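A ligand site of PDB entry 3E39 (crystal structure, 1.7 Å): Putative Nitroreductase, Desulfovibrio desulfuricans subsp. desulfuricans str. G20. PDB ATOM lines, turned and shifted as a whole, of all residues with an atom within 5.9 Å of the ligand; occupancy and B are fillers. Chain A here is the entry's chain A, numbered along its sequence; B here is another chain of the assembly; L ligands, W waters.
Water W1 bridges the side-chain hydroxyl (OG) of Ser 160 (2.7 Å) and an oxygen (O5) of the ligand (2.8 Å). Water W3 bridges O of Gly 44 of chain B and O3 of the ligand. Water W2 lies within hydrogen-bond range of the backbone carbonyl oxygen of Ser 17 (2.8 Å), an oxygen (O8) of the ligand (2.9 Å) and the backbone carbonyl oxygen of Ser 159 (3.2 Å). Water W6 lies within hydrogen-bond range of an oxygen (O6) of the ligand (2.9 Å) and the guanidinium group (NH1) of Arg 19 (2.9 Å). Water W4 lies within hydrogen-bond range of OE1 of Glu 124 (2.9 Å), N of Ile 125 (2.9 Å) and O2 of the ligand (2.9 Å).
The guanidinium group of Arg 162 sits at hydrogen-bond distance from the side-chain hydroxyl of Ser 160, at 2.9 Å. OD1 of Asn 46 of chain B lies within hydrogen-bond range of NH1 of Arg 162, at 3.3 Å. The backbone carbonyl oxygen (O) of Trp 40 of chain B is in hydrogen-bond range of the guanidinium group (NH2) of Arg 162 (3.1 Å). The guanidinium group (NE) of Arg 162 is in hydrogen-bond range of the backbone carbonyl oxygen (O) of Ala 41 of chain B (3.2 Å). The guanidinium group (NH2) of Arg 15 lies within hydrogen-bond range of the backbone carbonyl oxygen (O) of Trp 40 of chain B (3.3 Å). NZ of Lys 96 of chain B is in hydrogen-bond range of O of Gly 123, at 3.1 Å. The side-chain amide nitrogen (ND2) of Asn 46 of chain B lies within hydrogen-bond range of the backbone carbonyl oxygen (O) of Ser 161 (3.1 Å). The side-chain carboxylate (OD2) of Asp 97 of chain B sits at hydrogen-bond distance from the backbone NH (N) of Tyr 92 of chain B (2.6 Å).
O of Trp 121 lies close to N4 of the ligand, 3.0 Å away. Tyr 71 touches the ligand (CZ to N2, 3.5 Å). CD1 of Ile 74 touches O1 of the ligand, at 3.7 Å. Val 120 touches the ligand. Leu 122 touches the ligand. CB of Pro 42 of chain B touches O4 of the ligand (3.2 Å). Ser 43 of chain B touches the ligand. Asn 46 of chain B touches the ligand. OH of Tyr 92 of chain B touches C5 of the ligand, at 3.99 Å. CB of Lys 96 of chain B touches C7 of the ligand, 3.7 Å away. Gln 99 of chain B touches the ligand (OE1 to C7, 3.8 Å). Hydrophobic or aromatic side chains within 4 Å of the ligand: Tyr 71, Ile 74, Val 120, Trp 121, Leu 122 and Pro 42 of chain B. Of the 29 residues printed, 20 come within 4 Å of the ligand. The nearest printed residue that does not touch the ligand is Ser 159 (4.4 Å).
The backbone NH of Ser 17 lies within hydrogen-bond range of an oxygen (O8) of the ligand (2.9 Å). OG of Ser 17 is in hydrogen-bond range of O7 of the ligand (2.7 Å). The guanidinium group (NE) of Arg 19 is in hydrogen-bond range of an oxygen (O1) of the ligand, 2.7 Å away. NH2 of Arg 162 is in salt-bridge range of O9 of the ligand (2.8 Å). An oxygen (O9) of the ligand lies within salt-bridge range of the guanidinium group of Arg 16 (2.8 Å). The guanidinium group (NH1) of Arg 15 lies within salt-bridge range of an oxygen (O7) of the ligand, 2.8 Å away. N of Gly 123 sits at hydrogen-bond distance from N3 of the ligand (2.9 Å). N of Glu 124 is in hydrogen-bond range of O2 of the ligand (3.2 Å). The side-chain hydroxyl (OG) of Ser 160 lies within hydrogen-bond range of an oxygen (O6) of the ligand, at 3.3 Å. O of Gly 44 of chain B lies within hydrogen-bond range of O3 of the ligand (3.5 Å).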
ATOM      1  N   ARG A  15     -17.050   4.352  -9.159  1.00  0.00           N
ATOM      2  CA  ARG A  15     -15.805   5.057  -8.880  1.00  0.00           C
ATOM      3  C   ARG A  15     -15.055   4.319  -7.772  1.00  0.00           C
ATOM      4  O   ARG A  15     -15.609   4.093  -6.687  1.00  0.00           O
ATOM      5  CB  ARG A  15     -16.087   6.449  -8.362  1.00  0.00           C
ATOM      6  CG  ARG A  15     -14.843   7.231  -7.888  1.00  0.00           C
ATOM      7  CD  ARG A  15     -15.158   8.143  -6.648  1.00  0.00           C
ATOM      8  NE  ARG A  15     -15.754   7.347  -5.579  1.00  0.00           N
ATOM      9  CZ  ARG A  15     -15.086   6.635  -4.675  1.00  0.00           C
ATOM     10  NH1 ARG A  15     -13.750   6.585  -4.703  1.00  0.00           N
ATOM     11  NH2 ARG A  15     -15.748   5.915  -3.789  1.00  0.00           N
ATOM     12  N   ARG A  16     -13.786   4.005  -8.024  1.00  0.00           N
ATOM     13  CA  ARG A  16     -12.970   3.343  -7.024  1.00  0.00           C
ATOM     14  C   ARG A  16     -11.653   4.103  -6.826  1.00  0.00           C
ATOM     15  O   ARG A  16     -11.173   4.822  -7.724  1.00  0.00           O
ATOM     16  CB  ARG A  16     -12.590   1.917  -7.479  1.00  0.00           C
ATOM     17  CG  ARG A  16     -13.696   0.873  -7.576  1.00  0.00           C
ATOM     18  CD  ARG A  16     -14.011   0.165  -6.273  1.00  0.00           C
ATOM     19  NE  ARG A  16     -14.614   1.050  -5.272  1.00  0.00           N
ATOM     20  CZ  ARG A  16     -15.884   1.445  -5.305  1.00  0.00           C
ATOM     21  NH1 ARG A  16     -16.668   1.100  -6.304  1.00  0.00           N
ATOM     22  NH2 ARG A  16     -16.360   2.258  -4.355  1.00  0.00           N
ATOM     23  N   SER A  17     -11.070   3.925  -5.641  1.00  0.00           N
ATOM     24  CA  SER A  17      -9.731   4.423  -5.411  1.00  0.00           C
ATOM     25  C   SER A  17      -8.789   3.482  -6.192  1.00  0.00           C
ATOM     26  O   SER A  17      -8.712   2.290  -5.914  1.00  0.00           O
ATOM     27  CB  SER A  17      -9.356   4.400  -3.926  1.00  0.00           C
ATOM     28  OG  SER A  17     -10.062   5.374  -3.205  1.00  0.00           O
ATOM     29  N   ARG A  19      -4.879   2.989  -7.265  1.00  0.00           N
ATOM     30  CA  ARG A  19      -3.560   3.333  -6.754  1.00  0.00           C
ATOM     31  C   ARG A  19      -2.367   2.871  -7.605  1.00  0.00           C
ATOM     32  O   ARG A  19      -1.205   3.062  -7.196  1.00  0.00           O
ATOM     33  CB  ARG A  19      -3.452   2.748  -5.343  1.00  0.00           C
ATOM     34  CG  ARG A  19      -4.561   3.221  -4.375  1.00  0.00           C
ATOM     35  CD  ARG A  19      -4.494   2.545  -3.009  1.00  0.00           C
ATOM     36  NE  ARG A  19      -5.398   3.162  -2.021  1.00  0.00           N
ATOM     37  CZ  ARG A  19      -6.667   2.803  -1.824  1.00  0.00           C
ATOM     38  NH1 ARG A  19      -7.245   1.859  -2.562  1.00  0.00           N
ATOM     39  NH2 ARG A  19      -7.373   3.431  -0.925  1.00  0.00           N
ATOM     40  N   TYR A  71       2.655   7.028   1.714  1.00  0.00           N
ATOM     41  CA  TYR A  71       2.145   6.503   0.459  1.00  0.00           C
ATOM     42  C   TYR A  71       2.969   6.962  -0.744  1.00  0.00           C
ATOM     43  O   TYR A  71       2.444   7.368  -1.785  1.00  0.00           O
ATOM     44  CB  TYR A  71       0.688   6.897   0.274  1.00  0.00           C
ATOM     45  CG  TYR A  71      -0.208   6.319   1.322  1.00  0.00           C
ATOM     46  CD1 TYR A  71      -0.798   5.070   1.136  1.00  0.00           C
ATOM     47  CD2 TYR A  71      -0.476   6.998   2.514  1.00  0.00           C
ATOM     48  CE1 TYR A  71      -1.631   4.527   2.093  1.00  0.00           C
ATOM     49  CE2 TYR A  71      -1.298   6.456   3.481  1.00  0.00           C
ATOM     50  CZ  TYR A  71      -1.860   5.204   3.243  1.00  0.00           C
ATOM     51  OH  TYR A  71      -2.681   4.635   4.158  1.00  0.00           O
ATOM     52  N   ILE A  74       2.315   5.295  -4.316  1.00  0.00           N
ATOM     53  CA  ILE A  74       1.232   5.906  -5.066  1.00  0.00           C
ATOM     54  C   ILE A  74       1.733   7.212  -5.675  1.00  0.00           C
ATOM     55  O   ILE A  74       1.554   7.459  -6.874  1.00  0.00           O
ATOM     56  CB  ILE A  74       0.003   6.196  -4.145  1.00  0.00           C
ATOM     57  CG1 ILE A  74      -0.590   4.875  -3.613  1.00  0.00           C
ATOM     58  CG2 ILE A  74      -1.086   7.011  -4.921  1.00  0.00           C
ATOM     59  CD1 ILE A  74      -1.718   5.038  -2.584  1.00  0.00           C
ATOM     60  N   VAL A 120      -6.981   8.347  -6.786  1.00  0.00           N
ATOM     61  CA  VAL A 120      -7.138   8.114  -5.369  1.00  0.00           C
ATOM     62  C   VAL A 120      -6.952   9.410  -4.549  1.00  0.00           C
ATOM     63  O   VAL A 120      -6.024  10.227  -4.810  1.00  0.00           O
ATOM     64  CB  VAL A 120      -6.228   6.962  -4.828  1.00  0.00           C
ATOM     65  CG1 VAL A 120      -4.722   7.244  -5.112  1.00  0.00           C
ATOM     66  CG2 VAL A 120      -6.502   6.720  -3.336  1.00  0.00           C
ATOM     67  N   TRP A 121      -7.876   9.604  -3.609  1.00  0.00           N
ATOM     68  CA  TRP A 121      -7.885  10.716  -2.671  1.00  0.00           C
ATOM     69  C   TRP A 121      -6.825  10.385  -1.640  1.00  0.00           C
ATOM     70  O   TRP A 121      -6.915   9.358  -0.992  1.00  0.00           O
ATOM     71  CB  TRP A 121      -9.241  10.736  -1.983  1.00  0.00           C
ATOM     72  CG  TRP A 121      -9.517  11.823  -1.004  1.00  0.00           C
ATOM     73  CD1 TRP A 121      -8.642  12.441  -0.141  1.00  0.00           C
ATOM     74  CD2 TRP A 121     -10.803  12.365  -0.725  1.00  0.00           C
ATOM     75  NE1 TRP A 121      -9.316  13.343   0.644  1.00  0.00           N
ATOM     76  CE2 TRP A 121     -10.639  13.331   0.295  1.00  0.00           C
ATOM     77  CE3 TRP A 121     -12.075  12.129  -1.242  1.00  0.00           C
ATOM     78  CZ2 TRP A 121     -11.718  14.064   0.797  1.00  0.00           C
ATOM     79  CZ3 TRP A 121     -13.145  12.873  -0.739  1.00  0.00           C
ATOM     80  CH2 TRP A 121     -12.959  13.822   0.269  1.00  0.00           C
ATOM     81  N   LEU A 122      -5.814  11.232  -1.482  1.00  0.00           N
ATOM     82  CA  LEU A 122      -4.789  11.010  -0.482  1.00  0.00           C
ATOM     83  C   LEU A 122      -4.924  12.055   0.608  1.00  0.00           C
ATOM     84  O   LEU A 122      -4.840  13.248   0.322  1.00  0.00           O
ATOM     85  CB  LEU A 122      -3.391  11.082  -1.106  1.00  0.00           C
ATOM     86  CG  LEU A 122      -3.039  10.017  -2.138  1.00  0.00           C
ATOM     87  CD1 LEU A 122      -1.628  10.258  -2.701  1.00  0.00           C
ATOM     88  CD2 LEU A 122      -3.139   8.641  -1.563  1.00  0.00           C
ATOM     89  N   GLY A 123      -5.204  11.610   1.835  1.00  0.00           N
ATOM     90  CA  GLY A 123      -5.376  12.483   3.006  1.00  0.00           C
ATOM     91  C   GLY A 123      -4.342  12.305   4.108  1.00  0.00           C
ATOM     92  O   GLY A 123      -4.108  13.196   4.889  1.00  0.00           O
ATOM     93  N   GLU A 124      -3.712  11.144   4.181  1.00  0.00           N
ATOM     94  CA  GLU A 124      -2.645  10.988   5.173  1.00  0.00           C
ATOM     95  C   GLU A 124      -1.562  12.032   4.960  1.00  0.00           C
ATOM     96  O   GLU A 124      -0.936  12.501   5.924  1.00  0.00           O
ATOM     97  CB  GLU A 124      -2.100   9.564   5.092  1.00  0.00           C
ATOM     98  CG  GLU A 124      -0.791   9.324   5.835  1.00  0.00           C
ATOM     99  CD  GLU A 124       0.465   9.666   5.015  1.00  0.00           C
ATOM    100  OE1 GLU A 124       0.340  10.060   3.834  1.00  0.00           O
ATOM    101  OE2 GLU A 124       1.564   9.525   5.575  1.00  0.00           O
ATOM    102  N   ILE A 125      -1.372  12.458   3.715  1.00  0.00           N
ATOM    103  CA  ILE A 125      -0.330  13.386   3.366  1.00  0.00           C
ATOM    104  C   ILE A 125      -0.523  14.760   4.019  1.00  0.00           C
ATOM    105  O   ILE A 125       0.460  15.463   4.300  1.00  0.00           O
ATOM    106  CB  ILE A 125      -0.132  13.492   1.818  1.00  0.00           C
ATOM    107  CG1 ILE A 125       1.159  14.287   1.488  1.00  0.00           C
ATOM    108  CG2 ILE A 125      -1.383  14.073   1.074  1.00  0.00           C
ATOM    109  CD1 ILE A 125       1.643  14.074   0.076  1.00  0.00           C
ATOM    110  N   GLY A 158     -10.195  -1.328  -8.744  1.00  0.00           N
ATOM    111  CA  GLY A 158     -10.169  -1.238  -7.304  1.00  0.00           C
ATOM    112  C   GLY A 158     -11.246  -2.152  -6.782  1.00  0.00           C
ATOM    113  O   GLY A 158     -11.928  -2.836  -7.537  1.00  0.00           O
ATOM    114  N   SER A 159     -11.383  -2.164  -5.462  1.00  0.00           N
ATOM    115  CA  SER A 159     -12.456  -2.905  -4.817  1.00  0.00           C
ATOM    116  C   SER A 159     -12.681  -2.274  -3.450  1.00  0.00           C
ATOM    117  O   SER A 159     -11.729  -1.781  -2.821  1.00  0.00           O
ATOM    118  CB  SER A 159     -12.115  -4.400  -4.663  1.00  0.00           C
ATOM    119  OG  SER A 159     -11.230  -4.606  -3.565  1.00  0.00           O
ATOM    120  N   SER A 160     -13.924  -2.274  -2.999  1.00  0.00           N
ATOM    121  CA  SER A 160     -14.270  -1.735  -1.682  1.00  0.00           C
ATOM    122  C   SER A 160     -15.626  -2.301  -1.274  1.00  0.00           C
ATOM    123  O   SER A 160     -16.247  -3.078  -2.028  1.00  0.00           O
ATOM    124  CB  SER A 160     -14.309  -0.202  -1.718  1.00  0.00           C
ATOM    125  OG  SER A 160     -14.479   0.361  -0.438  1.00  0.00           O
ATOM    126  N   SER A 161     -16.086  -1.875  -0.109  1.00  0.00           N
ATOM    127  CA  SER A 161     -17.361  -2.320   0.434  1.00  0.00           C
ATOM    128  C   SER A 161     -18.020  -1.158   1.135  1.00  0.00           C
ATOM    129  O   SER A 161     -17.381  -0.177   1.481  1.00  0.00           O
ATOM    130  CB  SER A 161     -17.141  -3.457   1.431  1.00  0.00           C
ATOM    131  OG  SER A 161     -16.507  -3.054   2.642  1.00  0.00           O
ATOM    132  N   ARG A 162     -19.330  -1.212   1.245  1.00  0.00           N
ATOM    133  CA  ARG A 162     -20.053  -0.237   2.057  1.00  0.00           C
ATOM    134  C   ARG A 162     -21.047  -0.975   2.928  1.00  0.00           C
ATOM    135  O   ARG A 162     -21.534  -2.056   2.548  1.00  0.00           O
ATOM    136  CB  ARG A 162     -20.788   0.796   1.218  1.00  0.00           C
ATOM    137  CG  ARG A 162     -19.911   1.776   0.449  1.00  0.00           C
ATOM    138  CD  ARG A 162     -19.074   2.720   1.335  1.00  0.00           C
ATOM    139  NE  ARG A 162     -18.422   3.683   0.415  1.00  0.00           N
ATOM    140  CZ  ARG A 162     -17.330   3.431  -0.287  1.00  0.00           C
ATOM    141  NH1 ARG A 162     -16.669   2.287  -0.124  1.00  0.00           N
ATOM    142  NH2 ARG A 162     -16.850   4.338  -1.132  1.00  0.00           N
ATOM    143  N   TRP B  40     -22.046   5.659  -0.935  1.00  0.00           N
ATOM    144  CA  TRP B  40     -20.912   5.269  -1.758  1.00  0.00           C
ATOM    145  C   TRP B  40     -19.843   6.360  -1.937  1.00  0.00           C
ATOM    146  O   TRP B  40     -18.836   6.154  -2.591  1.00  0.00           O
ATOM    147  CB  TRP B  40     -21.364   4.655  -3.092  1.00  0.00           C
ATOM    148  CG  TRP B  40     -21.763   3.210  -2.898  1.00  0.00           C
ATOM    149  CD1 TRP B  40     -23.015   2.721  -2.680  1.00  0.00           C
ATOM    150  CD2 TRP B  40     -20.876   2.073  -2.876  1.00  0.00           C
ATOM    151  NE1 TRP B  40     -22.972   1.352  -2.533  1.00  0.00           N
ATOM    152  CE2 TRP B  40     -21.674   0.930  -2.644  1.00  0.00           C
ATOM    153  CE3 TRP B  40     -19.492   1.917  -3.033  1.00  0.00           C
ATOM    154  CZ2 TRP B  40     -21.120  -0.344  -2.545  1.00  0.00           C
ATOM    155  CZ3 TRP B  40     -18.960   0.660  -2.922  1.00  0.00           C
ATOM    156  CH2 TRP B  40     -19.760  -0.463  -2.678  1.00  0.00           C
ATOM    157  N   ALA B  41     -20.020   7.513  -1.289  1.00  0.00           N
ATOM    158  CA  ALA B  41     -18.937   8.479  -1.257  1.00  0.00           C
ATOM    159  C   ALA B  41     -17.820   7.767  -0.455  1.00  0.00           C
ATOM    160  O   ALA B  41     -18.091   6.894   0.413  1.00  0.00           O
ATOM    161  CB  ALA B  41     -19.364   9.801  -0.556  1.00  0.00           C
ATOM    162  N   PRO B  42     -16.567   8.166  -0.679  1.00  0.00           N
ATOM    163  CA  PRO B  42     -15.438   7.599   0.092  1.00  0.00           C
ATOM    164  C   PRO B  42     -15.295   8.210   1.511  1.00  0.00           C
ATOM    165  O   PRO B  42     -15.902   9.225   1.828  1.00  0.00           O
ATOM    166  CB  PRO B  42     -14.237   7.968  -0.774  1.00  0.00           C
ATOM    167  CG  PRO B  42     -14.653   9.265  -1.380  1.00  0.00           C
ATOM    168  CD  PRO B  42     -16.127   9.206  -1.614  1.00  0.00           C
ATOM    169  N   SER B  43     -14.478   7.571   2.342  1.00  0.00           N
ATOM    170  CA  SER B  43     -14.149   8.029   3.671  1.00  0.00           C
ATOM    171  C   SER B  43     -12.719   7.540   3.881  1.00  0.00           C
ATOM    172  O   SER B  43     -12.325   6.528   3.302  1.00  0.00           O
ATOM    173  CB  SER B  43     -15.122   7.512   4.737  1.00  0.00           C
ATOM    174  OG  SER B  43     -15.188   6.089   4.755  1.00  0.00           O
ATOM    175  N   GLY B  44     -11.959   8.259   4.685  1.00  0.00           N
ATOM    176  CA  GLY B  44     -10.507   8.004   4.889  1.00  0.00           C
ATOM    177  C   GLY B  44     -10.029   6.579   5.152  1.00  0.00           C
ATOM    178  O   GLY B  44      -9.019   6.135   4.582  1.00  0.00           O
ATOM    179  N   LEU B  45     -10.715   5.886   6.052  1.00  0.00           N
ATOM    180  CA  LEU B  45     -10.341   4.512   6.393  1.00  0.00           C
ATOM    181  C   LEU B  45     -11.439   3.561   6.001  1.00  0.00           C
ATOM    182  O   LEU B  45     -11.516   2.455   6.493  1.00  0.00           O
ATOM    183  CB  LEU B  45     -10.106   4.401   7.890  1.00  0.00           C
ATOM    184  CG  LEU B  45      -9.117   5.406   8.482  1.00  0.00           C
ATOM    185  CD1 LEU B  45      -9.081   5.271   9.986  1.00  0.00           C
ATOM    186  CD2 LEU B  45      -7.730   5.243   7.882  1.00  0.00           C
ATOM    187  N   ASN B  46     -12.264   3.966   5.034  1.00  0.00           N
ATOM    188  CA  ASN B  46     -13.519   3.259   4.767  1.00  0.00           C
ATOM    189  C   ASN B  46     -14.321   3.158   6.083  1.00  0.00           C
ATOM    190  O   ASN B  46     -15.080   2.183   6.295  1.00  0.00           O
ATOM    191  CB  ASN B  46     -13.359   1.895   4.066  1.00  0.00           C
ATOM    192  CG  ASN B  46     -14.651   1.446   3.395  1.00  0.00           C
ATOM    193  OD1 ASN B  46     -15.466   2.285   2.999  1.00  0.00           O
ATOM    194  ND2 ASN B  46     -14.838   0.131   3.256  1.00  0.00           N
ATOM    195  N   TYR B  92     -12.479   9.227  12.601  1.00  0.00           N
ATOM    196  CA  TYR B  92     -11.032   9.021  12.829  1.00  0.00           C
ATOM    197  C   TYR B  92     -10.259  10.347  12.810  1.00  0.00           C
ATOM    198  O   TYR B  92      -9.171  10.465  13.398  1.00  0.00           O
ATOM    199  CB  TYR B  92     -10.442   8.002  11.849  1.00  0.00           C
ATOM    200  CG  TYR B  92      -9.989   8.557  10.510  1.00  0.00           C
ATOM    201  CD1 TYR B  92     -10.902   8.951   9.557  1.00  0.00           C
ATOM    202  CD2 TYR B  92      -8.635   8.682  10.193  1.00  0.00           C
ATOM    203  CE1 TYR B  92     -10.496   9.432   8.325  1.00  0.00           C
ATOM    204  CE2 TYR B  92      -8.229   9.171   9.002  1.00  0.00           C
ATOM    205  CZ  TYR B  92      -9.149   9.543   8.057  1.00  0.00           C
ATOM    206  OH  TYR B  92      -8.764  10.032   6.827  1.00  0.00           O
ATOM    207  N   LYS B  96     -10.936  15.395   8.093  1.00  0.00           N
ATOM    208  CA  LYS B  96     -11.137  14.461   6.997  1.00  0.00           C
ATOM    209  C   LYS B  96     -12.539  13.817   7.011  1.00  0.00           C
ATOM    210  O   LYS B  96     -13.056  13.417   5.955  1.00  0.00           O
ATOM    211  CB  LYS B  96     -10.021  13.407   6.943  1.00  0.00           C
ATOM    212  CG  LYS B  96      -8.625  14.035   6.717  1.00  0.00           C
ATOM    213  CD  LYS B  96      -7.556  12.932   6.853  1.00  0.00           C
ATOM    214  CE  LYS B  96      -6.318  13.341   7.573  1.00  0.00           C
ATOM    215  NZ  LYS B  96      -5.406  12.150   7.550  1.00  0.00           N
ATOM    216  N   ASP B  97     -13.151  13.679   8.175  1.00  0.00           N
ATOM    217  CA  ASP B  97     -14.534  13.135   8.235  1.00  0.00           C
ATOM    218  C   ASP B  97     -15.571  14.196   7.764  1.00  0.00           C
ATOM    219  O   ASP B  97     -16.581  13.847   7.137  1.00  0.00           O
ATOM    220  CB  ASP B  97     -14.835  12.495   9.591  1.00  0.00           C
ATOM    221  CG  ASP B  97     -14.089  11.158   9.777  1.00  0.00           C
ATOM    222  OD1 ASP B  97     -14.002  10.381   8.798  1.00  0.00           O
ATOM    223  OD2 ASP B  97     -13.568  10.888  10.878  1.00  0.00           O
ATOM    224  N   GLN B  99     -14.751  16.380   5.462  1.00  0.00           N
ATOM    225  CA  GLN B  99     -14.553  16.348   4.006  1.00  0.00           C
ATOM    226  C   GLN B  99     -15.381  15.190   3.426  1.00  0.00           C
ATOM    227  O   GLN B  99     -16.033  15.309   2.382  1.00  0.00           O
ATOM    228  CB  GLN B  99     -13.086  16.115   3.659  1.00  0.00           C
ATOM    229  CG  GLN B  99     -12.165  17.270   4.013  1.00  0.00           C
ATOM    230  CD  GLN B  99     -10.717  16.912   3.829  1.00  0.00           C
ATOM    231  OE1 GLN B  99     -10.360  15.716   3.792  1.00  0.00           O
ATOM    232  NE2 GLN B  99      -9.862  17.936   3.656  1.00  0.00           N
ATOM    233  N   ALA B 100     -15.366  14.060   4.133  1.00  0.00           N
ATOM    234  CA  ALA B 100     -16.156  12.894   3.721  1.00  0.00           C
ATOM    235  C   ALA B 100     -17.656  13.182   3.672  1.00  0.00           C
ATOM    236  O   ALA B 100     -18.339  12.702   2.760  1.00  0.00           O
ATOM    237  CB  ALA B 100     -15.872  11.700   4.641  1.00  0.00           C
HETATM  238  N1  LIG L   1      -6.323   6.024   0.281  1.00  0.00           N
HETATM  239  C1  LIG L   1      -4.969   5.794   0.402  1.00  0.00           C
HETATM  240  O1  LIG L   1      -4.431   4.849  -0.149  1.00  0.00           O
HETATM  241  N2  LIG L   1      -4.180   6.664   1.134  1.00  0.00           N
HETATM  242  C2  LIG L   1      -4.694   7.767   1.775  1.00  0.00           C
HETATM  243  O2  LIG L   1      -3.913   8.625   2.236  1.00  0.00           O
HETATM  244  C3  LIG L   1      -6.068   8.003   1.676  1.00  0.00           C
HETATM  245  N3  LIG L   1      -6.601   9.105   2.307  1.00  0.00           N
HETATM  246  C4  LIG L   1      -7.961   9.384   2.200  1.00  0.00           C
HETATM  247  C5  LIG L   1      -8.484  10.494   2.871  1.00  0.00           C
HETATM  248  C6  LIG L   1      -9.847  10.803   2.767  1.00  0.00           C
HETATM  249  C7  LIG L   1     -10.430  11.892   3.630  1.00  0.00           C
HETATM  250  C8  LIG L   1     -10.681   9.960   2.008  1.00  0.00           C
HETATM  251  C9  LIG L   1     -12.149  10.289   1.860  1.00  0.00           C
HETATM  252  C10 LIG L   1     -10.155   8.838   1.366  1.00  0.00           C
HETATM  253  C11 LIG L   1      -8.783   8.532   1.450  1.00  0.00           C
HETATM  254  N4  LIG L   1      -8.226   7.394   0.796  1.00  0.00           N
HETATM  255  C12 LIG L   1      -6.868   7.135   0.914  1.00  0.00           C
HETATM  256  C13 LIG L   1      -9.060   6.462   0.021  1.00  0.00           C
HETATM  257  C14 LIG L   1      -9.909   5.547   0.923  1.00  0.00           C
HETATM  258  O3  LIG L   1      -9.097   4.533   1.489  1.00  0.00           O
HETATM  259  C15 LIG L   1     -11.015   4.919   0.092  1.00  0.00           C
HETATM  260  O4  LIG L   1     -11.829   5.960  -0.422  1.00  0.00           O
HETATM  261  C16 LIG L   1     -11.905   3.976   0.904  1.00  0.00           C
HETATM  262  O5  LIG L   1     -11.128   2.886   1.346  1.00  0.00           O
HETATM  263  C17 LIG L   1     -13.052   3.444   0.081  1.00  0.00           C
HETATM  264  O6  LIG L   1     -12.598   2.953  -1.168  1.00  0.00           O
HETATM  265  P1  LIG L   1     -13.137   3.436  -2.595  1.00  0.00           P
HETATM  266  O7  LIG L   1     -12.634   4.854  -2.795  1.00  0.00           O
HETATM  267  O8  LIG L   1     -12.626   2.462  -3.638  1.00  0.00           O
HETATM  268  O9  LIG L   1     -14.643   3.409  -2.494  1.00  0.00           O
HETATM  269  O   HOH W   1     -12.091   0.342   0.720  1.00  0.00           O
HETATM  270  O   HOH W   2     -10.471   0.693  -4.361  1.00  0.00           O
HETATM  271  O   HOH W   3      -7.002   4.903   3.329  1.00  0.00           O
HETATM  272  O   HOH W   4      -1.584  10.337   1.707  1.00  0.00           O
HETATM  273  O   HOH W   5      -3.872   1.854   0.858  1.00  0.00           O
HETATM  274  O   HOH W   6      -9.972   1.674  -1.470  1.00  0.00           O
